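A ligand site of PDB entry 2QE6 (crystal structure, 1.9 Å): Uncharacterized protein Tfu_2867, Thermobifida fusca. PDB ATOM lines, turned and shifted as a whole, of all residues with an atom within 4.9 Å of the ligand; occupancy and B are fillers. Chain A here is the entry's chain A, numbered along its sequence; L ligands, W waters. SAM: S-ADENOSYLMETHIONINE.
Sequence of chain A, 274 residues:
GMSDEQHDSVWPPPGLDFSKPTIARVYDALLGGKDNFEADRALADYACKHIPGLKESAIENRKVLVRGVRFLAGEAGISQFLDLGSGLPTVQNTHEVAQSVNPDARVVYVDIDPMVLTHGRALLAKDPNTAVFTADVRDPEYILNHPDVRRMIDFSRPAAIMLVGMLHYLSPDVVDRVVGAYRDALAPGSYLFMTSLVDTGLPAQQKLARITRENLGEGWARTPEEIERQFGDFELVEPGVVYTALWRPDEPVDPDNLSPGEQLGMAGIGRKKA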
ATOM      1  N   ILE A  23     -30.210  -9.334   8.889  1.00  0.00           N
ATOM      2  CA  ILE A  23     -29.733 -10.528   9.606  1.00  0.00           C
ATOM      3  C   ILE A  23     -29.306 -10.192  11.007  1.00  0.00           C
ATOM      4  O   ILE A  23     -29.746 -10.838  11.967  1.00  0.00           O
ATOM      5  CB  ILE A  23     -28.585 -11.278   8.857  1.00  0.00           C
ATOM      6  CG1 ILE A  23     -29.095 -11.823   7.495  1.00  0.00           C
ATOM      7  CG2 ILE A  23     -28.118 -12.440   9.726  1.00  0.00           C
ATOM      8  CD1 ILE A  23     -27.967 -12.175   6.393  1.00  0.00           C
ATOM      9  N   ALA A  24     -28.478  -9.174  11.155  1.00  0.00           N
ATOM     10  CA  ALA A  24     -27.992  -8.815  12.487  1.00  0.00           C
ATOM     11  C   ALA A  24     -29.115  -8.487  13.446  1.00  0.00           C
ATOM     12  O   ALA A  24     -29.097  -8.929  14.596  1.00  0.00           O
ATOM     13  CB  ALA A  24     -26.992  -7.625  12.410  1.00  0.00           C
ATOM     14  N   TYR A  27     -31.421 -11.554  14.497  1.00  0.00           N
ATOM     15  CA  TYR A  27     -30.688 -12.391  15.461  1.00  0.00           C
ATOM     16  C   TYR A  27     -30.659 -11.660  16.794  1.00  0.00           C
ATOM     17  O   TYR A  27     -30.895 -12.244  17.824  1.00  0.00           O
ATOM     18  CB  TYR A  27     -29.294 -12.623  14.931  1.00  0.00           C
ATOM     19  CG  TYR A  27     -28.441 -13.534  15.719  1.00  0.00           C
ATOM     20  CD1 TYR A  27     -28.586 -14.889  15.645  1.00  0.00           C
ATOM     21  CD2 TYR A  27     -27.431 -13.025  16.517  1.00  0.00           C
ATOM     22  CE1 TYR A  27     -27.747 -15.759  16.398  1.00  0.00           C
ATOM     23  CE2 TYR A  27     -26.595 -13.869  17.254  1.00  0.00           C
ATOM     24  CZ  TYR A  27     -26.759 -15.249  17.193  1.00  0.00           C
ATOM     25  OH  TYR A  27     -25.941 -16.097  17.903  1.00  0.00           O
ATOM     26  N   ASN A  61     -25.820 -20.906  20.276  1.00  0.00           N
ATOM     27  CA  ASN A  61     -24.756 -20.390  19.406  1.00  0.00           C
ATOM     28  C   ASN A  61     -23.907 -19.351  20.129  1.00  0.00           C
ATOM     29  O   ASN A  61     -22.675 -19.382  20.072  1.00  0.00           O
ATOM     30  CB  ASN A  61     -25.370 -19.832  18.122  1.00  0.00           C
ATOM     31  CG  ASN A  61     -24.350 -19.517  17.099  1.00  0.00           C
ATOM     32  OD1 ASN A  61     -23.592 -20.367  16.655  1.00  0.00           O
ATOM     33  ND2 ASN A  61     -24.335 -18.264  16.693  1.00  0.00           N
ATOM     34  N   ARG A  62     -24.556 -18.468  20.874  1.00  0.00           N
ATOM     35  CA  ARG A  62     -23.796 -17.531  21.721  1.00  0.00           C
ATOM     36  C   ARG A  62     -22.989 -18.235  22.793  1.00  0.00           C
ATOM     37  O   ARG A  62     -21.865 -17.857  23.029  1.00  0.00           O
ATOM     38  CB  ARG A  62     -24.701 -16.491  22.365  1.00  0.00           C
ATOM     39  CG  ARG A  62     -25.367 -15.611  21.328  1.00  0.00           C
ATOM     40  CD  ARG A  62     -24.349 -14.996  20.374  1.00  0.00           C
ATOM     41  NE  ARG A  62     -23.385 -14.176  21.113  1.00  0.00           N
ATOM     42  CZ  ARG A  62     -22.578 -13.265  20.577  1.00  0.00           C
ATOM     43  NH1 ARG A  62     -22.575 -13.051  19.273  1.00  0.00           N
ATOM     44  NH2 ARG A  62     -21.758 -12.570  21.378  1.00  0.00           N
ATOM     45  N   LEU A  65     -19.968 -19.774  21.186  1.00  0.00           N
ATOM     46  CA  LEU A  65     -19.058 -18.697  20.839  1.00  0.00           C
ATOM     47  C   LEU A  65     -18.170 -18.420  22.049  1.00  0.00           C
ATOM     48  O   LEU A  65     -16.952 -18.336  21.921  1.00  0.00           O
ATOM     49  CB  LEU A  65     -19.808 -17.423  20.444  1.00  0.00           C
ATOM     50  CG  LEU A  65     -19.017 -16.143  20.094  1.00  0.00           C
ATOM     51  CD1 LEU A  65     -19.926 -15.297  19.208  1.00  0.00           C
ATOM     52  CD2 LEU A  65     -18.538 -15.354  21.331  1.00  0.00           C
ATOM     53  N   ASP A  83     -13.300 -11.531  13.551  1.00  0.00           N
ATOM     54  CA  ASP A  83     -14.633 -12.024  13.831  1.00  0.00           C
ATOM     55  C   ASP A  83     -15.545 -11.533  12.707  1.00  0.00           C
ATOM     56  O   ASP A  83     -16.013 -10.370  12.709  1.00  0.00           O
ATOM     57  CB  ASP A  83     -15.074 -11.544  15.207  1.00  0.00           C
ATOM     58  CG  ASP A  83     -16.421 -12.125  15.684  1.00  0.00           C
ATOM     59  OD1 ASP A  83     -17.088 -12.914  14.952  1.00  0.00           O
ATOM     60  OD2 ASP A  83     -16.843 -11.746  16.821  1.00  0.00           O
ATOM     61  N   LEU A  84     -15.779 -12.433  11.742  1.00  0.00           N
ATOM     62  CA  LEU A  84     -16.487 -12.120  10.513  1.00  0.00           C
ATOM     63  C   LEU A  84     -17.988 -12.350  10.654  1.00  0.00           C
ATOM     64  O   LEU A  84     -18.425 -13.477  10.953  1.00  0.00           O
ATOM     65  CB  LEU A  84     -15.974 -13.009   9.393  1.00  0.00           C
ATOM     66  CG  LEU A  84     -14.463 -12.832   9.088  1.00  0.00           C
ATOM     67  CD1 LEU A  84     -14.034 -13.935   8.116  1.00  0.00           C
ATOM     68  CD2 LEU A  84     -14.117 -11.445   8.552  1.00  0.00           C
ATOM     69  N   GLY A  85     -18.778 -11.327  10.371  1.00  0.00           N
ATOM     70  CA  GLY A  85     -20.211 -11.395  10.591  1.00  0.00           C
ATOM     71  C   GLY A  85     -20.442 -11.338  12.078  1.00  0.00           C
ATOM     72  O   GLY A  85     -21.113 -12.183  12.621  1.00  0.00           O
ATOM     73  N   SER A  86     -19.866 -10.349  12.742  1.00  0.00           N
ATOM     74  CA  SER A  86     -19.832 -10.329  14.207  1.00  0.00           C
ATOM     75  C   SER A  86     -21.199 -10.249  14.879  1.00  0.00           C
ATOM     76  O   SER A  86     -21.364 -10.664  16.046  1.00  0.00           O
ATOM     77  CB  SER A  86     -19.047  -9.095  14.684  1.00  0.00           C
ATOM     78  OG  SER A  86     -19.665  -7.898  14.227  1.00  0.00           O
ATOM     79  N   GLY A  87     -22.155  -9.600  14.189  1.00  0.00           N
ATOM     80  CA  GLY A  87     -23.447  -9.247  14.770  1.00  0.00           C
ATOM     81  C   GLY A  87     -23.425  -8.074  15.728  1.00  0.00           C
ATOM     82  O   GLY A  87     -22.374  -7.477  15.993  1.00  0.00           O
ATOM     83  N   LEU A  88     -24.610  -7.750  16.252  1.00  0.00           N
ATOM     84  CA  LEU A  88     -24.761  -6.629  17.210  1.00  0.00           C
ATOM     85  C   LEU A  88     -24.386  -7.090  18.633  1.00  0.00           C
ATOM     86  O   LEU A  88     -24.341  -8.282  18.904  1.00  0.00           O
ATOM     87  CB  LEU A  88     -26.209  -6.145  17.126  1.00  0.00           C
ATOM     88  CG  LEU A  88     -26.572  -5.476  15.790  1.00  0.00           C
ATOM     89  CD1 LEU A  88     -28.065  -5.476  15.601  1.00  0.00           C
ATOM     90  CD2 LEU A  88     -26.063  -3.992  15.850  1.00  0.00           C
ATOM     91  N   VAL A 110     -16.150  -7.498  12.039  1.00  0.00           N
ATOM     92  CA  VAL A 110     -16.580  -7.086  10.702  1.00  0.00           C
ATOM     93  C   VAL A 110     -18.043  -7.480  10.547  1.00  0.00           C
ATOM     94  O   VAL A 110     -18.392  -8.614  10.862  1.00  0.00           O
ATOM     95  CB  VAL A 110     -15.731  -7.792   9.597  1.00  0.00           C
ATOM     96  CG1 VAL A 110     -16.151  -7.345   8.193  1.00  0.00           C
ATOM     97  CG2 VAL A 110     -14.228  -7.498   9.867  1.00  0.00           C
ATOM     98  N   ASP A 111     -18.881  -6.537  10.133  1.00  0.00           N
ATOM     99  CA  ASP A 111     -20.259  -6.824   9.826  1.00  0.00           C
ATOM    100  C   ASP A 111     -20.739  -5.946   8.690  1.00  0.00           C
ATOM    101  O   ASP A 111     -20.257  -4.874   8.497  1.00  0.00           O
ATOM    102  CB  ASP A 111     -21.177  -6.705  11.051  1.00  0.00           C
ATOM    103  CG  ASP A 111     -22.438  -7.588  10.938  1.00  0.00           C
ATOM    104  OD1 ASP A 111     -23.392  -7.216  10.241  1.00  0.00           O
ATOM    105  OD2 ASP A 111     -22.499  -8.656  11.565  1.00  0.00           O
ATOM    106  N   ILE A 112     -21.694  -6.453   7.941  1.00  0.00           N
ATOM    107  CA  ILE A 112     -22.285  -5.724   6.815  1.00  0.00           C
ATOM    108  C   ILE A 112     -23.362  -4.711   7.261  1.00  0.00           C
ATOM    109  O   ILE A 112     -23.585  -3.715   6.610  1.00  0.00           O
ATOM    110  CB  ILE A 112     -22.862  -6.725   5.757  1.00  0.00           C
ATOM    111  CG1 ILE A 112     -23.301  -6.002   4.484  1.00  0.00           C
ATOM    112  CG2 ILE A 112     -24.007  -7.560   6.362  1.00  0.00           C
ATOM    113  CD1 ILE A 112     -22.203  -5.224   3.811  1.00  0.00           C
ATOM    114  N   ASP A 113     -24.031  -4.990   8.378  1.00  0.00           N
ATOM    115  CA  ASP A 113     -25.039  -4.080   8.926  1.00  0.00           C
ATOM    116  C   ASP A 113     -24.340  -2.878   9.518  1.00  0.00           C
ATOM    117  O   ASP A 113     -23.649  -3.028  10.474  1.00  0.00           O
ATOM    118  CB  ASP A 113     -25.873  -4.804  10.022  1.00  0.00           C
ATOM    119  CG  ASP A 113     -27.150  -4.068  10.388  1.00  0.00           C
ATOM    120  OD1 ASP A 113     -27.146  -2.811  10.231  1.00  0.00           O
ATOM    121  OD2 ASP A 113     -28.134  -4.722  10.858  1.00  0.00           O
ATOM    122  N   ALA A 135     -18.144  -4.268   6.328  1.00  0.00           N
ATOM    123  CA  ALA A 135     -17.636  -4.794   5.094  1.00  0.00           C
ATOM    124  C   ALA A 135     -18.406  -6.055   4.784  1.00  0.00           C
ATOM    125  O   ALA A 135     -19.107  -6.611   5.638  1.00  0.00           O
ATOM    126  CB  ALA A 135     -16.141  -5.075   5.186  1.00  0.00           C
ATOM    127  N   ASP A 136     -18.261  -6.501   3.550  1.00  0.00           N
ATOM    128  CA  ASP A 136     -18.872  -7.757   3.111  1.00  0.00           C
ATOM    129  C   ASP A 136     -17.839  -8.875   3.109  1.00  0.00           C
ATOM    130  O   ASP A 136     -16.892  -8.876   2.322  1.00  0.00           O
ATOM    131  CB  ASP A 136     -19.429  -7.563   1.723  1.00  0.00           C
ATOM    132  CG  ASP A 136     -20.193  -8.735   1.233  1.00  0.00           C
ATOM    133  OD1 ASP A 136     -20.046  -9.830   1.753  1.00  0.00           O
ATOM    134  OD2 ASP A 136     -20.988  -8.531   0.301  1.00  0.00           O
ATOM    135  N   VAL A 137     -18.075  -9.869   3.963  1.00  0.00           N
ATOM    136  CA  VAL A 137     -17.229 -11.066   4.155  1.00  0.00           C
ATOM    137  C   VAL A 137     -16.952 -11.862   2.890  1.00  0.00           C
ATOM    138  O   VAL A 137     -15.957 -12.598   2.789  1.00  0.00           O
ATOM    139  CB  VAL A 137     -17.917 -11.928   5.264  1.00  0.00           C
ATOM    140  CG1 VAL A 137     -17.416 -13.371   5.308  1.00  0.00           C
ATOM    141  CG2 VAL A 137     -17.731 -11.205   6.581  1.00  0.00           C
ATOM    142  N   ARG A 138     -17.820 -11.696   1.889  1.00  0.00           N
ATOM    143  CA  ARG A 138     -17.624 -12.349   0.603  1.00  0.00           C
ATOM    144  C   ARG A 138     -16.537 -11.676  -0.241  1.00  0.00           C
ATOM    145  O   ARG A 138     -16.248 -12.127  -1.358  1.00  0.00           O
ATOM    146  CB  ARG A 138     -18.932 -12.387  -0.140  1.00  0.00           C
ATOM    147  CG  ARG A 138     -19.961 -13.238   0.576  1.00  0.00           C
ATOM    148  CD  ARG A 138     -21.285 -13.166  -0.131  1.00  0.00           C
ATOM    149  NE  ARG A 138     -21.837 -11.819  -0.033  1.00  0.00           N
ATOM    150  CZ  ARG A 138     -23.027 -11.448  -0.501  1.00  0.00           C
ATOM    151  NH1 ARG A 138     -23.820 -12.325  -1.100  1.00  0.00           N
ATOM    152  NH2 ARG A 138     -23.419 -10.187  -0.368  1.00  0.00           N
ATOM    153  N   VAL A 164     -18.631 -17.639  12.924  1.00  0.00           N
ATOM    154  CA  VAL A 164     -19.596 -18.135  13.863  1.00  0.00           C
ATOM    155  C   VAL A 164     -20.975 -17.525  13.465  1.00  0.00           C
ATOM    156  O   VAL A 164     -21.073 -16.325  13.240  1.00  0.00           O
ATOM    157  CB  VAL A 164     -19.147 -17.810  15.339  1.00  0.00           C
ATOM    158  CG1 VAL A 164     -20.243 -18.187  16.376  1.00  0.00           C
ATOM    159  CG2 VAL A 164     -17.843 -18.552  15.680  1.00  0.00           C
ATOM    160  N   GLY A 165     -21.975 -18.387  13.304  1.00  0.00           N
ATOM    161  CA  GLY A 165     -23.299 -17.979  12.862  1.00  0.00           C
ATOM    162  C   GLY A 165     -23.371 -17.333  11.495  1.00  0.00           C
ATOM    163  O   GLY A 165     -24.311 -16.557  11.217  1.00  0.00           O
ATOM    164  N   MET A 166     -22.386 -17.658  10.651  1.00  0.00           N
ATOM    165  CA  MET A 166     -22.092 -16.893   9.406  1.00  0.00           C
ATOM    166  C   MET A 166     -22.038 -17.875   8.203  1.00  0.00           C
ATOM    167  O   MET A 166     -22.405 -17.520   7.057  1.00  0.00           O
ATOM    168  CB  MET A 166     -20.755 -16.091   9.667  1.00  0.00           C
ATOM    169  CG  MET A 166     -20.127 -14.962   8.718  1.00  0.00           C
ATOM    170  SD  MET A 166     -21.449 -13.971   7.786  1.00  0.00           S
ATOM    171  CE  MET A 166     -20.952 -14.564   6.004  1.00  0.00           C
ATOM    172  N   TYR A 169     -24.866 -18.174   5.603  1.00  0.00           N
ATOM    173  CA  TYR A 169     -25.166 -17.026   4.729  1.00  0.00           C
ATOM    174  C   TYR A 169     -24.273 -16.979   3.494  1.00  0.00           C
ATOM    175  O   TYR A 169     -24.361 -16.014   2.710  1.00  0.00           O
ATOM    176  CB  TYR A 169     -25.070 -15.686   5.526  1.00  0.00           C
ATOM    177  CG  TYR A 169     -26.028 -15.667   6.695  1.00  0.00           C
ATOM    178  CD1 TYR A 169     -27.404 -15.814   6.500  1.00  0.00           C
ATOM    179  CD2 TYR A 169     -25.556 -15.574   7.980  1.00  0.00           C
ATOM    180  CE1 TYR A 169     -28.284 -15.877   7.571  1.00  0.00           C
ATOM    181  CE2 TYR A 169     -26.406 -15.618   9.050  1.00  0.00           C
ATOM    182  CZ  TYR A 169     -27.776 -15.745   8.851  1.00  0.00           C
ATOM    183  OH  TYR A 169     -28.576 -15.789   9.950  1.00  0.00           O
HETATM  184  N   SAM L   1     -21.459 -14.090  14.565  1.00  0.00           N
HETATM  185  CA  SAM L   1     -22.594 -13.723  15.503  1.00  0.00           C
HETATM  186  C   SAM L   1     -22.979 -14.944  16.322  1.00  0.00           C
HETATM  187  O   SAM L   1     -23.491 -14.807  17.421  1.00  0.00           O
HETATM  188  OXT SAM L   1     -22.815 -16.078  15.861  1.00  0.00           O
HETATM  189  CB  SAM L   1     -23.895 -13.221  14.843  1.00  0.00           C
HETATM  190  CG  SAM L   1     -24.626 -14.223  13.936  1.00  0.00           C
HETATM  191  SD  SAM L   1     -26.037 -13.563  12.986  1.00  0.00           S
HETATM  192  CE  SAM L   1     -25.926 -11.871  13.627  1.00  0.00           C
HETATM  193  C5' SAM L   1     -25.133 -13.321  11.444  1.00  0.00           C
HETATM  194  C4' SAM L   1     -24.310 -12.044  11.197  1.00  0.00           C
HETATM  195  O4' SAM L   1     -23.530 -12.204  10.013  1.00  0.00           O
HETATM  196  C3' SAM L   1     -25.163 -10.786  10.966  1.00  0.00           C
HETATM  197  O3' SAM L   1     -24.752  -9.728  11.805  1.00  0.00           O
HETATM  198  C2' SAM L   1     -24.996 -10.427   9.499  1.00  0.00           C
HETATM  199  O2' SAM L   1     -25.192  -9.038   9.191  1.00  0.00           O
HETATM  200  C1' SAM L   1     -23.606 -10.992   9.250  1.00  0.00           C
HETATM  201  N9  SAM L   1     -23.414 -11.273   7.829  1.00  0.00           N
HETATM  202  C8  SAM L   1     -24.090 -12.168   6.993  1.00  0.00           C
HETATM  203  N7  SAM L   1     -23.557 -12.088   5.749  1.00  0.00           N
HETATM  204  C5  SAM L   1     -22.550 -11.169   5.789  1.00  0.00           C
HETATM  205  C6  SAM L   1     -21.657 -10.721   4.801  1.00  0.00           C
HETATM  206  N6  SAM L   1     -21.763 -11.205   3.530  1.00  0.00           N
HETATM  207  N1  SAM L   1     -20.722  -9.774   5.167  1.00  0.00           N
HETATM  208  C2  SAM L   1     -20.631  -9.266   6.481  1.00  0.00           C
HETATM  209  N3  SAM L   1     -21.523  -9.703   7.449  1.00  0.00           N
HETATM  210  C4  SAM L   1     -22.447 -10.656   7.094  1.00  0.00           C
HETATM  211  O   HOH W   1     -19.251 -13.976  16.117  1.00  0.00           O
HETATM  212  O   HOH W   2     -27.490  -7.903   8.547  1.00  0.00           O
HETATM  213  O   HOH W   3     -23.684 -13.276   3.084  1.00  0.00           O
HETATM  214  O   HOH W   4     -26.740  -9.635  15.869  1.00  0.00           O
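ND2 of Asn 61 sits close to OXT of the ligand (2.8 Å). The backbone NH (N) of Ile 112 sits close to a nitrogen (N3) of the ligand (3.3 Å). The guanidinium group (NH1) of Arg 62 lies close to an oxygen (O) of the ligand, 2.7 Å away. OH of Tyr 27 lies close to O of the ligand (2.8 Å). The backbone NH of Val 137 lies close to a nitrogen (N1) of the ligand, at 2.9 Å. The side-chain carboxylate (OD2) of Asp 111 sits close to an oxygen (O3') of the ligand (2.5 Å). The side-chain sulfur (SD) of Met 166 lies close to a nitrogen (N9) of the ligand. O of Gly 85 sits close to N of the ligand, at 2.7 Å. A nitrogen (N) of the ligand sits close to the backbone carbonyl oxygen (O) of Val 164 (2.6 Å). OD1 of Asp 136 lies close to N6 of the ligand, at 2.8 Å.
OD2 of Asp 136 lies within salt-bridge range of NH2 of Arg 138 (3.0 Å). The side-chain carboxylate of Asp 111 is in hydrogen-bond range of the backbone NH of Asp 113, at 3.0 Å. The backbone carbonyl oxygen (O) of Ala 135 lies within hydrogen-bond range of the backbone NH (N) of Ile 112 (3.5 Å). The backbone carbonyl oxygen of Val 110 is in hydrogen-bond range of the backbone NH of Ser 86. The backbone NH of Gly 85 sits at hydrogen-bond distance from the backbone carbonyl oxygen of Val 110 (2.8 Å). OD2 of Asp 111 is in hydrogen-bond range of N of Ser 86 (3.3 Å). The side-chain amide nitrogen (ND2) of Asn 61 lies within hydrogen-bond range of the side-chain hydroxyl (OH) of Tyr 27 (3.0 Å). The side-chain carboxylate of Asp 111 lies within hydrogen-bond range of the backbone NH of Gly 87, 2.8 Å away.
CG2 of Ile 23 touches C5' of the ligand, 3.6 Å away. Ala 24 touches the ligand (CB to O3', 3.1 Å). O of Ser 86 touches CA of the ligand, 3.3 Å away. Gly 87 touches the ligand (CA to O3', 3.3 Å). O of Ala 135 touches C2 of the ligand, 3.2 Å away. Arg 138 touches the ligand. Gly 165 touches the ligand. CE2 of Tyr 169 touches C5' of the ligand, 3.6 Å away. Hydrophobic or aromatic side chains that line the ligand: Ile 23, Ala 24, Tyr 27, Ile 112, Val 137, Val 164, Met 166 and Tyr 169. Of the 24 residues printed, 18 come within 4 Å of the ligand.
Water W4 lies within hydrogen-bond range of the backbone carbonyl oxygen (O) of Ala 24 (2.8 Å) and the backbone NH (N) of Leu 88 (2.9 Å).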
